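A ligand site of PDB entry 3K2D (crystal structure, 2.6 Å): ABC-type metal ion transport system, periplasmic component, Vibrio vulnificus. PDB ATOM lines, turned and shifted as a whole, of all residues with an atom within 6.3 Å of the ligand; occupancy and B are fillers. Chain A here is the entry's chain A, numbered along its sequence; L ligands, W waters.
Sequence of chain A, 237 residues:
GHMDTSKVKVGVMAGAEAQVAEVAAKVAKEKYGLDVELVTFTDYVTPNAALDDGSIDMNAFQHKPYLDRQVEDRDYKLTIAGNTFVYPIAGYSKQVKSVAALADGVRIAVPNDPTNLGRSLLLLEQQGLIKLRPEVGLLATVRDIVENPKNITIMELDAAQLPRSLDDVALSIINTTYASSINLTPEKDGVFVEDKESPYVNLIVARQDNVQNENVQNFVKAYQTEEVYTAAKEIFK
The backbone carbonyl oxygen (O) of Tyr 87 lies within hydrogen-bond range of the guanidinium group (NH2) of Arg 119 (3.1 Å). O of Tyr 200 is in hydrogen-bond range of ND2 of Asn 202. The backbone carbonyl oxygen (O) of Phe 85 sits at hydrogen-bond distance from the backbone NH (N) of Asn 202 (2.7 Å). ND1 of His 63 lies within hydrogen-bond range of N of Tyr 66, at 3.2 Å. OH of Tyr 66 is in hydrogen-bond range of O of Tyr 44, at 3.2 Å. The side-chain carboxylate of Glu 17 is in hydrogen-bond range of the side-chain hydroxyl of Thr 177 (2.6 Å). NE2 of His 63 is in hydrogen-bond range of OD1 of Asn 116. The side-chain amide nitrogen (ND2) of Asn 116 sits at hydrogen-bond distance from the side-chain carboxylate (OD2) of Asp 113 (2.6 Å).
Merely in contact with the ligand: Tyr 44, Phe 61, Gln 62, Tyr 66 and Tyr 87. Hydrophobic or aromatic side chains within 4 Å of the ligand: Tyr 44, His 63, Tyr 66 and Tyr 87. Of the 23 residues printed, 11 come within 4 Å of the ligand.
Water W4 lies within hydrogen-bond range of an oxygen (O1) of the ligand (2.6 Å), the backbone NH (N) of Tyr 87 (2.8 Å), the backbone carbonyl oxygen (O) of Tyr 200 (2.8 Å) and the guanidinium group (NH2) of Arg 119 (3.2 Å). Water W3 lies within hydrogen-bond range of O2 of the ligand (2.6 Å), O of Tyr 87 (2.6 Å) and N of Thr 176 (3.0 Å). Water W1 lies within hydrogen-bond range of a nitrogen (N1) of the ligand (3.0 Å), the side-chain hydroxyl (OG1) of Thr 177 (3.1 Å) and the backbone NH (N) of Thr 176 (3.5 Å). Water W2 lies within hydrogen-bond range of the side-chain carboxylate (OE1) of Glu 17 (2.7 Å), the backbone carbonyl oxygen (O) of Phe 61 (2.8 Å), a nitrogen (N1) of the ligand (3.1 Å) and the side-chain hydroxyl (OG1) of Thr 177 (3.1 Å).
An oxygen (O2) of the ligand lies within salt-bridge range of the guanidinium group (NH1) of Arg 119. ND2 of Asn 202 lies within hydrogen-bond range of O1 of the ligand (3.2 Å). N1 of the ligand lies within hydrogen-bond range of OG1 of Thr 177, 3.3 Å away. The side-chain amide oxygen of Asn 175 sits close to an oxygen (O2) of the ligand, at 3.3 Å. A ring nitrogen (NE2) of His 63 sits close to a sulfur (S1) of the ligand (3.4 Å). A sulfur (S1) of the ligand lies close to the side-chain amide nitrogen (ND2) of Asn 116.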
ATOM      1  N   GLU A  17     -27.166 -27.913 -11.506  1.00  0.00           N
ATOM      2  CA  GLU A  17     -27.861 -26.636 -11.486  1.00  0.00           C
ATOM      3  C   GLU A  17     -28.697 -26.392 -10.229  1.00  0.00           C
ATOM      4  O   GLU A  17     -28.828 -25.263  -9.771  1.00  0.00           O
ATOM      5  CB  GLU A  17     -28.695 -26.481 -12.752  1.00  0.00           C
ATOM      6  CG  GLU A  17     -27.845 -26.065 -13.939  1.00  0.00           C
ATOM      7  CD  GLU A  17     -28.610 -25.998 -15.252  1.00  0.00           C
ATOM      8  OE1 GLU A  17     -29.756 -25.510 -15.256  1.00  0.00           O
ATOM      9  OE2 GLU A  17     -28.046 -26.421 -16.281  1.00  0.00           O
ATOM     10  N   TYR A  44     -36.775 -30.241 -20.100  1.00  0.00           N
ATOM     11  CA  TYR A  44     -36.831 -28.824 -20.458  1.00  0.00           C
ATOM     12  C   TYR A  44     -38.219 -28.265 -20.778  1.00  0.00           C
ATOM     13  O   TYR A  44     -38.481 -27.083 -20.530  1.00  0.00           O
ATOM     14  CB  TYR A  44     -35.927 -28.500 -21.652  1.00  0.00           C
ATOM     15  CG  TYR A  44     -34.434 -28.489 -21.365  1.00  0.00           C
ATOM     16  CD1 TYR A  44     -33.934 -28.186 -20.099  1.00  0.00           C
ATOM     17  CD2 TYR A  44     -33.517 -28.733 -22.390  1.00  0.00           C
ATOM     18  CE1 TYR A  44     -32.553 -28.117 -19.856  1.00  0.00           C
ATOM     19  CE2 TYR A  44     -32.157 -28.675 -22.167  1.00  0.00           C
ATOM     20  CZ  TYR A  44     -31.671 -28.369 -20.903  1.00  0.00           C
ATOM     21  OH  TYR A  44     -30.313 -28.281 -20.722  1.00  0.00           O
ATOM     22  N   PHE A  61     -33.523 -21.958 -15.961  1.00  0.00           N
ATOM     23  CA  PHE A  61     -32.991 -23.103 -16.703  1.00  0.00           C
ATOM     24  C   PHE A  61     -32.813 -22.885 -18.215  1.00  0.00           C
ATOM     25  O   PHE A  61     -32.186 -23.707 -18.889  1.00  0.00           O
ATOM     26  CB  PHE A  61     -33.953 -24.287 -16.528  1.00  0.00           C
ATOM     27  CG  PHE A  61     -35.189 -24.159 -17.375  1.00  0.00           C
ATOM     28  CD1 PHE A  61     -36.128 -23.165 -17.126  1.00  0.00           C
ATOM     29  CD2 PHE A  61     -35.376 -24.973 -18.489  1.00  0.00           C
ATOM     30  CE1 PHE A  61     -37.217 -22.967 -17.972  1.00  0.00           C
ATOM     31  CE2 PHE A  61     -36.453 -24.792 -19.342  1.00  0.00           C
ATOM     32  CZ  PHE A  61     -37.383 -23.788 -19.089  1.00  0.00           C
ATOM     33  N   GLN A  62     -33.325 -21.788 -18.762  1.00  0.00           N
ATOM     34  CA  GLN A  62     -33.242 -21.589 -20.208  1.00  0.00           C
ATOM     35  C   GLN A  62     -32.526 -20.340 -20.682  1.00  0.00           C
ATOM     36  O   GLN A  62     -32.176 -19.461 -19.901  1.00  0.00           O
ATOM     37  CB  GLN A  62     -34.653 -21.534 -20.789  1.00  0.00           C
ATOM     38  CG  GLN A  62     -35.375 -20.226 -20.467  1.00  0.00           C
ATOM     39  CD  GLN A  62     -36.882 -20.385 -20.455  1.00  0.00           C
ATOM     40  OE1 GLN A  62     -37.497 -20.728 -21.470  1.00  0.00           O
ATOM     41  NE2 GLN A  62     -37.487 -20.127 -19.297  1.00  0.00           N
ATOM     42  N   HIS A  63     -32.298 -20.288 -21.996  1.00  0.00           N
ATOM     43  CA  HIS A  63     -31.710 -19.111 -22.629  1.00  0.00           C
ATOM     44  C   HIS A  63     -32.821 -18.456 -23.456  1.00  0.00           C
ATOM     45  O   HIS A  63     -33.863 -19.045 -23.683  1.00  0.00           O
ATOM     46  CB  HIS A  63     -30.474 -19.468 -23.475  1.00  0.00           C
ATOM     47  CG  HIS A  63     -30.614 -20.672 -24.350  1.00  0.00           C
ATOM     48  ND1 HIS A  63     -31.595 -20.785 -25.326  1.00  0.00           N
ATOM     49  CD2 HIS A  63     -29.835 -21.781 -24.482  1.00  0.00           C
ATOM     50  CE1 HIS A  63     -31.402 -21.898 -26.017  1.00  0.00           C
ATOM     51  NE2 HIS A  63     -30.347 -22.517 -25.523  1.00  0.00           N
ATOM     52  N   TYR A  66     -34.534 -20.284 -26.553  1.00  0.00           N
ATOM     53  CA  TYR A  66     -35.425 -21.346 -26.114  1.00  0.00           C
ATOM     54  C   TYR A  66     -36.769 -20.837 -25.586  1.00  0.00           C
ATOM     55  O   TYR A  66     -37.812 -21.427 -25.851  1.00  0.00           O
ATOM     56  CB  TYR A  66     -34.743 -22.188 -25.047  1.00  0.00           C
ATOM     57  CG  TYR A  66     -35.569 -23.393 -24.658  1.00  0.00           C
ATOM     58  CD1 TYR A  66     -36.557 -23.289 -23.688  1.00  0.00           C
ATOM     59  CD2 TYR A  66     -35.356 -24.624 -25.261  1.00  0.00           C
ATOM     60  CE1 TYR A  66     -37.312 -24.392 -23.328  1.00  0.00           C
ATOM     61  CE2 TYR A  66     -36.103 -25.731 -24.907  1.00  0.00           C
ATOM     62  CZ  TYR A  66     -37.087 -25.609 -23.943  1.00  0.00           C
ATOM     63  OH  TYR A  66     -37.846 -26.704 -23.593  1.00  0.00           O
ATOM     64  N   LEU A  67     -36.723 -19.767 -24.800  1.00  0.00           N
ATOM     65  CA  LEU A  67     -37.925 -19.187 -24.240  1.00  0.00           C
ATOM     66  C   LEU A  67     -38.814 -18.599 -25.355  1.00  0.00           C
ATOM     67  O   LEU A  67     -40.008 -18.887 -25.415  1.00  0.00           O
ATOM     68  CB  LEU A  67     -37.533 -18.087 -23.246  1.00  0.00           C
ATOM     69  CG  LEU A  67     -38.610 -17.134 -22.739  1.00  0.00           C
ATOM     70  CD1 LEU A  67     -39.659 -17.869 -21.924  1.00  0.00           C
ATOM     71  CD2 LEU A  67     -37.931 -16.046 -21.913  1.00  0.00           C
ATOM     72  N   PHE A  85     -26.090 -17.595 -15.816  1.00  0.00           N
ATOM     73  CA  PHE A  85     -24.799 -17.901 -16.427  1.00  0.00           C
ATOM     74  C   PHE A  85     -24.881 -18.422 -17.852  1.00  0.00           C
ATOM     75  O   PHE A  85     -25.947 -18.776 -18.344  1.00  0.00           O
ATOM     76  CB  PHE A  85     -24.041 -18.937 -15.594  1.00  0.00           C
ATOM     77  CG  PHE A  85     -23.866 -18.559 -14.164  1.00  0.00           C
ATOM     78  CD1 PHE A  85     -23.114 -17.450 -13.812  1.00  0.00           C
ATOM     79  CD2 PHE A  85     -24.478 -19.308 -13.171  1.00  0.00           C
ATOM     80  CE1 PHE A  85     -22.956 -17.089 -12.482  1.00  0.00           C
ATOM     81  CE2 PHE A  85     -24.332 -18.962 -11.830  1.00  0.00           C
ATOM     82  CZ  PHE A  85     -23.570 -17.847 -11.487  1.00  0.00           C
ATOM     83  N   VAL A  86     -23.724 -18.450 -18.489  1.00  0.00           N
ATOM     84  CA  VAL A  86     -23.575 -18.966 -19.844  1.00  0.00           C
ATOM     85  C   VAL A  86     -22.942 -20.341 -19.647  1.00  0.00           C
ATOM     86  O   VAL A  86     -22.036 -20.487 -18.828  1.00  0.00           O
ATOM     87  CB  VAL A  86     -22.597 -18.132 -20.677  1.00  0.00           C
ATOM     88  CG1 VAL A  86     -22.486 -18.716 -22.071  1.00  0.00           C
ATOM     89  CG2 VAL A  86     -23.040 -16.684 -20.725  1.00  0.00           C
ATOM     90  N   TYR A  87     -23.419 -21.332 -20.378  1.00  0.00           N
ATOM     91  CA  TYR A  87     -22.864 -22.659 -20.265  1.00  0.00           C
ATOM     92  C   TYR A  87     -22.443 -23.100 -21.668  1.00  0.00           C
ATOM     93  O   TYR A  87     -23.152 -23.837 -22.341  1.00  0.00           O
ATOM     94  CB  TYR A  87     -23.904 -23.622 -19.677  1.00  0.00           C
ATOM     95  CG  TYR A  87     -24.274 -23.354 -18.231  1.00  0.00           C
ATOM     96  CD1 TYR A  87     -23.414 -23.685 -17.186  1.00  0.00           C
ATOM     97  CD2 TYR A  87     -25.512 -22.778 -17.914  1.00  0.00           C
ATOM     98  CE1 TYR A  87     -23.782 -23.455 -15.855  1.00  0.00           C
ATOM     99  CE2 TYR A  87     -25.884 -22.540 -16.593  1.00  0.00           C
ATOM    100  CZ  TYR A  87     -25.015 -22.880 -15.566  1.00  0.00           C
ATOM    101  OH  TYR A  87     -25.411 -22.663 -14.263  1.00  0.00           O
ATOM    102  N   PRO A  88     -21.279 -22.629 -22.133  1.00  0.00           N
ATOM    103  CA  PRO A  88     -20.786 -22.989 -23.461  1.00  0.00           C
ATOM    104  C   PRO A  88     -20.908 -24.493 -23.711  1.00  0.00           C
ATOM    105  O   PRO A  88     -20.157 -25.294 -23.157  1.00  0.00           O
ATOM    106  CB  PRO A  88     -19.337 -22.516 -23.421  1.00  0.00           C
ATOM    107  CG  PRO A  88     -19.445 -21.268 -22.582  1.00  0.00           C
ATOM    108  CD  PRO A  88     -20.331 -21.725 -21.452  1.00  0.00           C
ATOM    109  N   ILE A  89     -21.850 -24.878 -24.558  1.00  0.00           N
ATOM    110  CA  ILE A  89     -22.089 -26.279 -24.854  1.00  0.00           C
ATOM    111  C   ILE A  89     -20.873 -26.909 -25.523  1.00  0.00           C
ATOM    112  O   ILE A  89     -20.121 -26.241 -26.219  1.00  0.00           O
ATOM    113  CB  ILE A  89     -23.340 -26.438 -25.761  1.00  0.00           C
ATOM    114  CG1 ILE A  89     -23.867 -27.872 -25.664  1.00  0.00           C
ATOM    115  CG2 ILE A  89     -23.016 -26.077 -27.213  1.00  0.00           C
ATOM    116  CD1 ILE A  89     -25.382 -27.955 -25.590  1.00  0.00           C
ATOM    117  N   ASP A 113     -34.733 -30.224 -29.621  1.00  0.00           N
ATOM    118  CA  ASP A 113     -35.589 -29.058 -29.575  1.00  0.00           C
ATOM    119  C   ASP A 113     -34.924 -28.096 -30.570  1.00  0.00           C
ATOM    120  O   ASP A 113     -33.710 -28.057 -30.692  1.00  0.00           O
ATOM    121  CB  ASP A 113     -35.654 -28.477 -28.154  1.00  0.00           C
ATOM    122  CG  ASP A 113     -34.310 -28.176 -27.597  1.00  0.00           C
ATOM    123  OD1 ASP A 113     -33.604 -29.119 -27.185  1.00  0.00           O
ATOM    124  OD2 ASP A 113     -33.941 -26.986 -27.576  1.00  0.00           O
ATOM    125  N   THR A 115     -34.136 -24.715 -30.875  1.00  0.00           N
ATOM    126  CA  THR A 115     -33.056 -23.761 -30.630  1.00  0.00           C
ATOM    127  C   THR A 115     -31.744 -24.435 -30.261  1.00  0.00           C
ATOM    128  O   THR A 115     -30.677 -23.917 -30.562  1.00  0.00           O
ATOM    129  CB  THR A 115     -33.408 -22.742 -29.528  1.00  0.00           C
ATOM    130  OG1 THR A 115     -33.588 -23.401 -28.275  1.00  0.00           O
ATOM    131  CG2 THR A 115     -34.667 -21.968 -29.913  1.00  0.00           C
ATOM    132  N   ASN A 116     -31.803 -25.579 -29.594  1.00  0.00           N
ATOM    133  CA  ASN A 116     -30.561 -26.252 -29.246  1.00  0.00           C
ATOM    134  C   ASN A 116     -30.065 -27.122 -30.403  1.00  0.00           C
ATOM    135  O   ASN A 116     -28.886 -27.451 -30.482  1.00  0.00           O
ATOM    136  CB  ASN A 116     -30.735 -27.064 -27.955  1.00  0.00           C
ATOM    137  CG  ASN A 116     -30.841 -26.167 -26.729  1.00  0.00           C
ATOM    138  OD1 ASN A 116     -29.882 -25.476 -26.357  1.00  0.00           O
ATOM    139  ND2 ASN A 116     -32.019 -26.151 -26.113  1.00  0.00           N
ATOM    140  N   ARG A 119     -28.303 -24.584 -32.488  1.00  0.00           N
ATOM    141  CA  ARG A 119     -27.081 -24.234 -31.786  1.00  0.00           C
ATOM    142  C   ARG A 119     -26.003 -25.285 -32.064  1.00  0.00           C
ATOM    143  O   ARG A 119     -24.836 -24.958 -32.335  1.00  0.00           O
ATOM    144  CB  ARG A 119     -27.377 -24.168 -30.301  1.00  0.00           C
ATOM    145  CG  ARG A 119     -26.230 -23.792 -29.411  1.00  0.00           C
ATOM    146  CD  ARG A 119     -26.685 -23.879 -27.961  1.00  0.00           C
ATOM    147  NE  ARG A 119     -25.661 -23.483 -27.014  1.00  0.00           N
ATOM    148  CZ  ARG A 119     -25.813 -23.522 -25.698  1.00  0.00           C
ATOM    149  NH1 ARG A 119     -26.959 -23.936 -25.176  1.00  0.00           N
ATOM    150  NH2 ARG A 119     -24.816 -23.155 -24.893  1.00  0.00           N
ATOM    151  N   ILE A 174     -23.724 -32.302 -25.815  1.00  0.00           N
ATOM    152  CA  ILE A 174     -24.606 -32.385 -24.665  1.00  0.00           C
ATOM    153  C   ILE A 174     -24.649 -31.099 -23.856  1.00  0.00           C
ATOM    154  O   ILE A 174     -23.621 -30.488 -23.608  1.00  0.00           O
ATOM    155  CB  ILE A 174     -24.120 -33.503 -23.707  1.00  0.00           C
ATOM    156  CG1 ILE A 174     -23.905 -34.797 -24.498  1.00  0.00           C
ATOM    157  CG2 ILE A 174     -25.117 -33.708 -22.592  1.00  0.00           C
ATOM    158  CD1 ILE A 174     -23.315 -35.947 -23.685  1.00  0.00           C
ATOM    159  N   ASN A 175     -25.865 -30.695 -23.447  1.00  0.00           N
ATOM    160  CA  ASN A 175     -26.040 -29.500 -22.625  1.00  0.00           C
ATOM    161  C   ASN A 175     -25.288 -29.807 -21.326  1.00  0.00           C
ATOM    162  O   ASN A 175     -25.332 -30.949 -20.840  1.00  0.00           O
ATOM    163  CB  ASN A 175     -27.533 -29.286 -22.292  1.00  0.00           C
ATOM    164  CG  ASN A 175     -28.380 -28.997 -23.524  1.00  0.00           C
ATOM    165  OD1 ASN A 175     -28.410 -27.873 -24.026  1.00  0.00           O
ATOM    166  ND2 ASN A 175     -29.076 -30.013 -24.009  1.00  0.00           N
ATOM    167  N   THR A 176     -24.591 -28.830 -20.760  1.00  0.00           N
ATOM    168  CA  THR A 176     -23.848 -29.059 -19.528  1.00  0.00           C
ATOM    169  C   THR A 176     -24.789 -29.505 -18.406  1.00  0.00           C
ATOM    170  O   THR A 176     -24.387 -30.169 -17.456  1.00  0.00           O
ATOM    171  CB  THR A 176     -23.089 -27.781 -19.084  1.00  0.00           C
ATOM    172  OG1 THR A 176     -22.103 -27.435 -20.077  1.00  0.00           O
ATOM    173  CG2 THR A 176     -22.395 -27.999 -17.762  1.00  0.00           C
ATOM    174  N   THR A 177     -26.059 -29.145 -18.542  1.00  0.00           N
ATOM    175  CA  THR A 177     -27.092 -29.502 -17.587  1.00  0.00           C
ATOM    176  C   THR A 177     -27.100 -30.991 -17.337  1.00  0.00           C
ATOM    177  O   THR A 177     -27.367 -31.448 -16.230  1.00  0.00           O
ATOM    178  CB  THR A 177     -28.491 -29.152 -18.121  1.00  0.00           C
ATOM    179  OG1 THR A 177     -28.563 -27.748 -18.401  1.00  0.00           O
ATOM    180  CG2 THR A 177     -29.562 -29.533 -17.108  1.00  0.00           C
ATOM    181  N   TYR A 200     -26.656 -17.556 -25.798  1.00  0.00           N
ATOM    182  CA  TYR A 200     -27.225 -18.554 -24.903  1.00  0.00           C
ATOM    183  C   TYR A 200     -27.089 -18.368 -23.394  1.00  0.00           C
ATOM    184  O   TYR A 200     -27.095 -19.352 -22.659  1.00  0.00           O
ATOM    185  CB  TYR A 200     -26.700 -19.922 -25.304  1.00  0.00           C
ATOM    186  CG  TYR A 200     -26.918 -20.211 -26.762  1.00  0.00           C
ATOM    187  CD1 TYR A 200     -28.192 -20.477 -27.250  1.00  0.00           C
ATOM    188  CD2 TYR A 200     -25.855 -20.161 -27.667  1.00  0.00           C
ATOM    189  CE1 TYR A 200     -28.404 -20.705 -28.616  1.00  0.00           C
ATOM    190  CE2 TYR A 200     -26.062 -20.384 -29.012  1.00  0.00           C
ATOM    191  CZ  TYR A 200     -27.330 -20.648 -29.492  1.00  0.00           C
ATOM    192  OH  TYR A 200     -27.509 -20.908 -30.829  1.00  0.00           O
ATOM    193  N   VAL A 201     -26.967 -17.138 -22.920  1.00  0.00           N
ATOM    194  CA  VAL A 201     -26.855 -16.946 -21.482  1.00  0.00           C
ATOM    195  C   VAL A 201     -28.171 -17.354 -20.849  1.00  0.00           C
ATOM    196  O   VAL A 201     -29.247 -17.017 -21.358  1.00  0.00           O
ATOM    197  CB  VAL A 201     -26.585 -15.472 -21.103  1.00  0.00           C
ATOM    198  CG1 VAL A 201     -27.780 -14.593 -21.512  1.00  0.00           C
ATOM    199  CG2 VAL A 201     -26.362 -15.366 -19.603  1.00  0.00           C
ATOM    200  N   ASN A 202     -28.103 -18.097 -19.748  1.00  0.00           N
ATOM    201  CA  ASN A 202     -29.314 -18.529 -19.068  1.00  0.00           C
ATOM    202  C   ASN A 202     -30.034 -17.397 -18.353  1.00  0.00           C
ATOM    203  O   ASN A 202     -29.497 -16.303 -18.187  1.00  0.00           O
ATOM    204  CB  ASN A 202     -29.016 -19.673 -18.109  1.00  0.00           C
ATOM    205  CG  ASN A 202     -28.742 -20.981 -18.831  1.00  0.00           C
ATOM    206  OD1 ASN A 202     -28.773 -22.047 -18.235  1.00  0.00           O
ATOM    207  ND2 ASN A 202     -28.472 -20.892 -20.131  1.00  0.00           N
HETATM  208  N1  LIG L   1     -28.956 -24.834 -19.867  1.00  0.00           N
HETATM  209  C1  LIG L   1     -28.865 -25.045 -21.364  1.00  0.00           C
HETATM  210  C2  LIG L   1     -27.536 -24.568 -21.809  1.00  0.00           C
HETATM  211  O1  LIG L   1     -27.085 -23.482 -21.340  1.00  0.00           O
HETATM  212  C3  LIG L   1     -29.870 -24.247 -22.164  1.00  0.00           C
HETATM  213  C4  LIG L   1     -31.270 -24.583 -21.909  1.00  0.00           C
HETATM  214  S1  LIG L   1     -32.320 -24.021 -23.202  1.00  0.00           S
HETATM  215  C5  LIG L   1     -33.728 -24.692 -22.387  1.00  0.00           C
HETATM  216  O2  LIG L   1     -26.909 -25.236 -22.643  1.00  0.00           O
HETATM  217  O   HOH W   1     -26.224 -26.026 -19.558  1.00  0.00           O
HETATM  218  O   HOH W   2     -30.851 -25.842 -17.690  1.00  0.00           O
HETATM  219  O   HOH W   3     -24.564 -26.035 -21.947  1.00  0.00           O
HETATM  220  O   HOH W   4     -25.507 -21.658 -22.176  1.00  0.00           O
